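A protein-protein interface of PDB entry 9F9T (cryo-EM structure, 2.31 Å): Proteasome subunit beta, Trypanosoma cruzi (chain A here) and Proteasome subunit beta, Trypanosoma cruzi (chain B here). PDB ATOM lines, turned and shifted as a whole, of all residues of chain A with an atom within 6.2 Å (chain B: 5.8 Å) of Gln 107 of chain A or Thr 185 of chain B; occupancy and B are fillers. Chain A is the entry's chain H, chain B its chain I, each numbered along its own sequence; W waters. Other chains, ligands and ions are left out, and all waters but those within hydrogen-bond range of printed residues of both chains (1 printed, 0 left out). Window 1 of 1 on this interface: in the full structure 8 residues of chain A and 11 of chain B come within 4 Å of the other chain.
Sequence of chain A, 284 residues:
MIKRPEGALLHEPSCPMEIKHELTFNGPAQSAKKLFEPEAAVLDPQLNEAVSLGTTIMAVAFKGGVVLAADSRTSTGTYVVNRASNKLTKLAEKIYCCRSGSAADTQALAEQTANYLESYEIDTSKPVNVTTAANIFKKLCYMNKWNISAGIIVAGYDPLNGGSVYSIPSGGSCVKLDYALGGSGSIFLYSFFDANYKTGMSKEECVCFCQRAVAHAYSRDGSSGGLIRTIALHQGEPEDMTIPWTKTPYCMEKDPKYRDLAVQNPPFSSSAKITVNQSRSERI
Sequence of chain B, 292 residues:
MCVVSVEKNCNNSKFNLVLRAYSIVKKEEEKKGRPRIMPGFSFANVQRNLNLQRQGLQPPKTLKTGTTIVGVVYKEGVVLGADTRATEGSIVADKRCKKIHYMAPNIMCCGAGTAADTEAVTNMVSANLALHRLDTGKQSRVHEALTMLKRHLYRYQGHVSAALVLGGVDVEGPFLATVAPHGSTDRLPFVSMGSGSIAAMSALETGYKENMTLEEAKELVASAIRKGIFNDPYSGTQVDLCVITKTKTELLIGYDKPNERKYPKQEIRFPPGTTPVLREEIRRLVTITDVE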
ATOM      1  N   ARG A  99      23.388 -16.611   5.623  1.00  0.00           N
ATOM      2  CA  ARG A  99      23.908 -17.164   6.842  1.00  0.00           C
ATOM      3  C   ARG A  99      24.763 -16.159   7.573  1.00  0.00           C
ATOM      4  O   ARG A  99      25.572 -15.518   6.962  1.00  0.00           O
ATOM      5  CB  ARG A  99      24.787 -18.367   6.540  1.00  0.00           C
ATOM      6  CG  ARG A  99      24.027 -19.546   5.937  1.00  0.00           C
ATOM      7  CD  ARG A  99      24.872 -20.773   5.585  1.00  0.00           C
ATOM      8  NE  ARG A  99      25.955 -20.562   4.602  1.00  0.00           N
ATOM      9  CZ  ARG A  99      27.192 -20.372   5.035  1.00  0.00           C
ATOM     10  NH1 ARG A  99      28.217 -20.163   4.219  1.00  0.00           N
ATOM     11  NH2 ARG A  99      27.375 -20.343   6.344  1.00  0.00           N
ATOM     12  N   SER A 102      28.098 -18.585  13.559  1.00  0.00           N
ATOM     13  CA  SER A 102      28.908 -19.759  13.400  1.00  0.00           C
ATOM     14  C   SER A 102      28.716 -20.325  12.025  1.00  0.00           C
ATOM     15  O   SER A 102      27.589 -20.628  11.658  1.00  0.00           O
ATOM     16  CB  SER A 102      28.462 -20.759  14.421  1.00  0.00           C
ATOM     17  OG  SER A 102      29.034 -22.056  14.210  1.00  0.00           O
ATOM     18  N   ALA A 103      29.788 -20.545  11.275  1.00  0.00           N
ATOM     19  CA  ALA A 103      29.611 -21.157   9.964  1.00  0.00           C
ATOM     20  C   ALA A 103      29.252 -22.633  10.099  1.00  0.00           C
ATOM     21  O   ALA A 103      28.329 -23.100   9.440  1.00  0.00           O
ATOM     22  CB  ALA A 103      30.837 -20.933   9.120  1.00  0.00           C
ATOM     23  N   ALA A 104      29.864 -23.344  11.038  1.00  0.00           N
ATOM     24  CA  ALA A 104      29.536 -24.755  11.284  1.00  0.00           C
ATOM     25  C   ALA A 104      28.054 -24.992  11.525  1.00  0.00           C
ATOM     26  O   ALA A 104      27.433 -25.674  10.711  1.00  0.00           O
ATOM     27  CB  ALA A 104      30.317 -25.232  12.445  1.00  0.00           C
ATOM     28  N   ASP A 105      27.440 -24.240  12.462  1.00  0.00           N
ATOM     29  CA  ASP A 105      25.994 -24.285  12.697  1.00  0.00           C
ATOM     30  C   ASP A 105      25.144 -23.938  11.462  1.00  0.00           C
ATOM     31  O   ASP A 105      24.176 -24.632  11.117  1.00  0.00           O
ATOM     32  CB  ASP A 105      25.602 -23.409  13.885  1.00  0.00           C
ATOM     33  CG  ASP A 105      26.253 -23.768  15.227  1.00  0.00           C
ATOM     34  OD1 ASP A 105      26.423 -25.053  15.579  1.00  0.00           O
ATOM     35  OD2 ASP A 105      26.590 -22.800  15.970  1.00  0.00           O
ATOM     36  N   THR A 106      25.404 -22.833  10.795  1.00  0.00           N
ATOM     37  CA  THR A 106      24.479 -22.424   9.731  1.00  0.00           C
ATOM     38  C   THR A 106      24.613 -23.247   8.466  1.00  0.00           C
ATOM     39  O   THR A 106      23.720 -23.262   7.629  1.00  0.00           O
ATOM     40  CB  THR A 106      24.841 -20.998   9.308  1.00  0.00           C
ATOM     41  OG1 THR A 106      26.228 -20.946   8.984  1.00  0.00           O
ATOM     42  CG2 THR A 106      24.650 -19.987  10.427  1.00  0.00           C
ATOM     43  N   GLN A 107      25.784 -23.839   8.235  1.00  0.00           N
ATOM     44  CA  GLN A 107      25.949 -24.831   7.170  1.00  0.00           C
ATOM     45  C   GLN A 107      25.128 -26.085   7.500  1.00  0.00           C
ATOM     46  O   GLN A 107      24.535 -26.643   6.604  1.00  0.00           O
ATOM     47  CB  GLN A 107      27.431 -25.232   6.974  1.00  0.00           C
ATOM     48  CG  GLN A 107      28.339 -24.175   6.371  1.00  0.00           C
ATOM     49  CD  GLN A 107      29.769 -24.654   6.167  1.00  0.00           C
ATOM     50  OE1 GLN A 107      30.064 -25.852   6.198  1.00  0.00           O
ATOM     51  NE2 GLN A 107      30.681 -23.715   5.984  1.00  0.00           N
ATOM     52  N   ALA A 108      25.172 -26.567   8.743  1.00  0.00           N
ATOM     53  CA  ALA A 108      24.431 -27.771   9.123  1.00  0.00           C
ATOM     54  C   ALA A 108      22.928 -27.513   9.085  1.00  0.00           C
ATOM     55  O   ALA A 108      22.236 -28.324   8.524  1.00  0.00           O
ATOM     56  CB  ALA A 108      24.780 -28.274  10.500  1.00  0.00           C
ATOM     57  N   LEU A 109      22.434 -26.363   9.573  1.00  0.00           N
ATOM     58  CA  LEU A 109      20.998 -26.104   9.505  1.00  0.00           C
ATOM     59  C   LEU A 109      20.548 -25.826   8.088  1.00  0.00           C
ATOM     60  O   LEU A 109      19.409 -26.109   7.774  1.00  0.00           O
ATOM     61  CB  LEU A 109      20.562 -25.018  10.489  1.00  0.00           C
ATOM     62  CG  LEU A 109      20.969 -25.253  11.968  1.00  0.00           C
ATOM     63  CD1 LEU A 109      20.233 -24.331  12.888  1.00  0.00           C
ATOM     64  CD2 LEU A 109      20.749 -26.667  12.512  1.00  0.00           C
ATOM     65  N   ALA A 110      21.376 -25.293   7.196  1.00  0.00           N
ATOM     66  CA  ALA A 110      20.848 -25.012   5.875  1.00  0.00           C
ATOM     67  C   ALA A 110      20.715 -26.306   5.079  1.00  0.00           C
ATOM     68  O   ALA A 110      19.793 -26.445   4.237  1.00  0.00           O
ATOM     69  CB  ALA A 110      21.744 -24.083   5.170  1.00  0.00           C
ATOM     70  N   GLU A 111      21.686 -27.207   5.360  1.00  0.00           N
ATOM     71  CA  GLU A 111      21.790 -28.462   4.646  1.00  0.00           C
ATOM     72  C   GLU A 111      20.550 -29.270   5.021  1.00  0.00           C
ATOM     73  O   GLU A 111      19.774 -29.655   4.181  1.00  0.00           O
ATOM     74  CB  GLU A 111      23.104 -29.199   4.979  1.00  0.00           C
ATOM     75  CG  GLU A 111      24.352 -28.818   4.150  1.00  0.00           C
ATOM     76  CD  GLU A 111      25.762 -28.927   4.803  1.00  0.00           C
ATOM     77  OE1 GLU A 111      25.930 -29.420   5.980  1.00  0.00           O
ATOM     78  OE2 GLU A 111      26.754 -28.451   4.163  1.00  0.00           O
ATOM     79  N   GLN A 112      20.268 -29.284   6.312  1.00  0.00           N
ATOM     80  CA  GLN A 112      19.097 -29.939   6.844  1.00  0.00           C
ATOM     81  C   GLN A 112      17.796 -29.331   6.352  1.00  0.00           C
ATOM     82  O   GLN A 112      16.904 -30.022   5.906  1.00  0.00           O
ATOM     83  CB  GLN A 112      19.173 -29.950   8.356  1.00  0.00           C
ATOM     84  CG  GLN A 112      18.481 -31.144   8.968  1.00  0.00           C
ATOM     85  CD  GLN A 112      18.655 -31.104  10.468  1.00  0.00           C
ATOM     86  OE1 GLN A 112      17.795 -31.588  11.219  1.00  0.00           O
ATOM     87  NE2 GLN A 112      19.753 -30.482  10.907  1.00  0.00           N
ATOM     88  N   LEU B 146      34.342 -35.089   2.096  1.00  0.00           N
ATOM     89  CA  LEU B 146      34.194 -33.829   2.794  1.00  0.00           C
ATOM     90  C   LEU B 146      32.957 -33.889   3.676  1.00  0.00           C
ATOM     91  O   LEU B 146      33.018 -33.527   4.869  1.00  0.00           O
ATOM     92  CB  LEU B 146      34.049 -32.685   1.779  1.00  0.00           C
ATOM     93  CG  LEU B 146      34.015 -31.307   2.469  1.00  0.00           C
ATOM     94  CD1 LEU B 146      35.264 -31.128   3.308  1.00  0.00           C
ATOM     95  CD2 LEU B 146      33.914 -30.100   1.495  1.00  0.00           C
ATOM     96  N   LYS B 150      32.517 -33.743   7.718  1.00  0.00           N
ATOM     97  CA  LYS B 150      31.807 -32.676   8.406  1.00  0.00           C
ATOM     98  C   LYS B 150      30.650 -33.208   9.263  1.00  0.00           C
ATOM     99  O   LYS B 150      30.462 -32.719  10.380  1.00  0.00           O
ATOM    100  CB  LYS B 150      31.415 -31.584   7.404  1.00  0.00           C
ATOM    101  CG  LYS B 150      30.062 -31.757   6.748  1.00  0.00           C
ATOM    102  CD  LYS B 150      29.798 -30.822   5.575  1.00  0.00           C
ATOM    103  CE  LYS B 150      30.197 -29.390   5.822  1.00  0.00           C
ATOM    104  NZ  LYS B 150      29.461 -28.812   6.956  1.00  0.00           N
ATOM    105  N   ALA B 177      39.672 -28.763  -0.030  1.00  0.00           N
ATOM    106  CA  ALA B 177      38.891 -28.110   0.971  1.00  0.00           C
ATOM    107  C   ALA B 177      39.510 -28.181   2.352  1.00  0.00           C
ATOM    108  O   ALA B 177      40.319 -29.040   2.551  1.00  0.00           O
ATOM    109  CB  ALA B 177      37.542 -28.690   0.931  1.00  0.00           C
ATOM    110  N   THR B 178      39.176 -27.223   3.239  1.00  0.00           N
ATOM    111  CA  THR B 178      39.475 -27.356   4.649  1.00  0.00           C
ATOM    112  C   THR B 178      38.279 -27.793   5.467  1.00  0.00           C
ATOM    113  O   THR B 178      37.174 -27.484   5.138  1.00  0.00           O
ATOM    114  CB  THR B 178      39.943 -26.071   5.290  1.00  0.00           C
ATOM    115  OG1 THR B 178      38.912 -25.095   5.263  1.00  0.00           O
ATOM    116  CG2 THR B 178      41.133 -25.444   4.592  1.00  0.00           C
ATOM    117  N   VAL B 179      38.508 -28.578   6.511  1.00  0.00           N
ATOM    118  CA  VAL B 179      37.499 -28.909   7.501  1.00  0.00           C
ATOM    119  C   VAL B 179      38.017 -28.581   8.892  1.00  0.00           C
ATOM    120  O   VAL B 179      38.929 -29.212   9.390  1.00  0.00           O
ATOM    121  CB  VAL B 179      37.155 -30.398   7.450  1.00  0.00           C
ATOM    122  CG1 VAL B 179      35.844 -30.739   8.172  1.00  0.00           C
ATOM    123  CG2 VAL B 179      37.113 -30.884   6.025  1.00  0.00           C
ATOM    124  N   ALA B 180      37.398 -27.594   9.527  1.00  0.00           N
ATOM    125  CA  ALA B 180      37.649 -27.201  10.904  1.00  0.00           C
ATOM    126  C   ALA B 180      36.992 -28.158  11.910  1.00  0.00           C
ATOM    127  O   ALA B 180      36.095 -28.918  11.611  1.00  0.00           O
ATOM    128  CB  ALA B 180      37.105 -25.839  11.019  1.00  0.00           C
ATOM    129  N   GLY B 183      33.148 -28.476  12.467  1.00  0.00           N
ATOM    130  CA  GLY B 183      32.403 -29.111  11.368  1.00  0.00           C
ATOM    131  C   GLY B 183      32.123 -28.176  10.198  1.00  0.00           C
ATOM    132  O   GLY B 183      31.316 -28.488   9.345  1.00  0.00           O
ATOM    133  N   SER B 184      32.863 -27.096  10.076  1.00  0.00           N
ATOM    134  CA  SER B 184      32.630 -26.223   8.949  1.00  0.00           C
ATOM    135  C   SER B 184      33.627 -26.515   7.849  1.00  0.00           C
ATOM    136  O   SER B 184      34.816 -26.616   8.106  1.00  0.00           O
ATOM    137  CB  SER B 184      32.753 -24.744   9.337  1.00  0.00           C
ATOM    138  OG  SER B 184      34.088 -24.341   9.613  1.00  0.00           O
ATOM    139  N   THR B 185      33.144 -26.434   6.616  1.00  0.00           N
ATOM    140  CA  THR B 185      33.954 -26.687   5.453  1.00  0.00           C
ATOM    141  C   THR B 185      34.043 -25.479   4.574  1.00  0.00           C
ATOM    142  O   THR B 185      33.127 -24.700   4.593  1.00  0.00           O
ATOM    143  CB  THR B 185      33.346 -27.743   4.546  1.00  0.00           C
ATOM    144  OG1 THR B 185      32.036 -27.324   4.162  1.00  0.00           O
ATOM    145  CG2 THR B 185      33.320 -29.097   5.217  1.00  0.00           C
ATOM    146  N   ASP B 186      35.110 -25.422   3.777  1.00  0.00           N
ATOM    147  CA  ASP B 186      35.408 -24.351   2.824  1.00  0.00           C
ATOM    148  C   ASP B 186      36.227 -24.890   1.651  1.00  0.00           C
ATOM    149  O   ASP B 186      37.353 -25.334   1.799  1.00  0.00           O
ATOM    150  CB  ASP B 186      36.300 -23.284   3.439  1.00  0.00           C
ATOM    151  CG  ASP B 186      35.612 -22.446   4.502  1.00  0.00           C
ATOM    152  OD1 ASP B 186      34.405 -22.040   4.275  1.00  0.00           O
ATOM    153  OD2 ASP B 186      36.306 -22.123   5.522  1.00  0.00           O
ATOM    154  N   ARG B 187      35.656 -24.889   0.500  1.00  0.00           N
ATOM    155  CA  ARG B 187      36.357 -25.245  -0.683  1.00  0.00           C
ATOM    156  C   ARG B 187      37.013 -24.014  -1.270  1.00  0.00           C
ATOM    157  O   ARG B 187      36.346 -23.019  -1.484  1.00  0.00           O
ATOM    158  CB  ARG B 187      35.276 -25.849  -1.575  1.00  0.00           C
ATOM    159  CG  ARG B 187      35.734 -25.844  -3.014  1.00  0.00           C
ATOM    160  CD  ARG B 187      34.916 -26.716  -3.930  1.00  0.00           C
ATOM    161  NE  ARG B 187      35.700 -26.904  -5.144  1.00  0.00           N
ATOM    162  CZ  ARG B 187      35.305 -27.682  -6.126  1.00  0.00           C
ATOM    163  NH1 ARG B 187      34.012 -27.911  -6.295  1.00  0.00           N
ATOM    164  NH2 ARG B 187      36.198 -28.145  -6.986  1.00  0.00           N
HETATM  165  O   HOH W   1      28.691 -28.034   9.393  1.00  0.00           O
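Water W1 lies within hydrogen-bond range of O of Gly 183 of chain B (2.7 Å), NZ of Lys 150 of chain B (2.7 Å) and O of Ala 104 of chain A (3.0 Å).
OE1 of Glu 111 of chain A lies within salt-bridge range of NZ of Lys 150 of chain B, 3.7 Å away.
OE1 of Gln 107 of chain A sits at hydrogen-bond distance from NZ of Lys 150 of chain B, 3.1 Å away.
NE2 of Gln 107 of chain A sits at hydrogen-bond distance from O of Thr 185 of chain B (3.0 Å).
Of the 12 printed residues of chain A, 3 touch a printed residue of chain B.
Hydrophobic or aromatic side chains of chain A that line the printed part of chain B: Ala 104.
Of the 11 printed residues of chain B, 3 touch a printed residue of chain A.
Among the printed residues, Asp or Glu carboxylates within 4 Å of a Lys or Arg side-chain nitrogen of the other chain: Glu 111 of chain A with Lys 150 of chain B.
NZ of Lys 150 of chain B lies within hydrogen-bond range of O of Gly 183 of chain B (3.0 Å).
Printed residues of chain B within 4 Å of Gln 107 of chain A: Lys 150 (3.1 Å), Ser 184 (3.8 Å) and Thr 185 (3.0 Å).
Of the printed residues of chain A, Lys 150 of chain B touches Gln 107 and Glu 111.
Of the printed residues of chain B, Ala 104 of chain A touches Ser 184.
Of the printed residues of chain B, Glu 111 of chain A touches Lys 150 (3.7 Å).
Of the printed residues of chain A, Ser 184 of chain B touches Ala 104 (3.6 Å) and Gln 107 (3.8 Å).
Among the printed residues, merely in contact across the chains: Ala 104 of chain A with Ser 184 of chain B and Gln 107 of chain A with Ser 184 of chain B.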
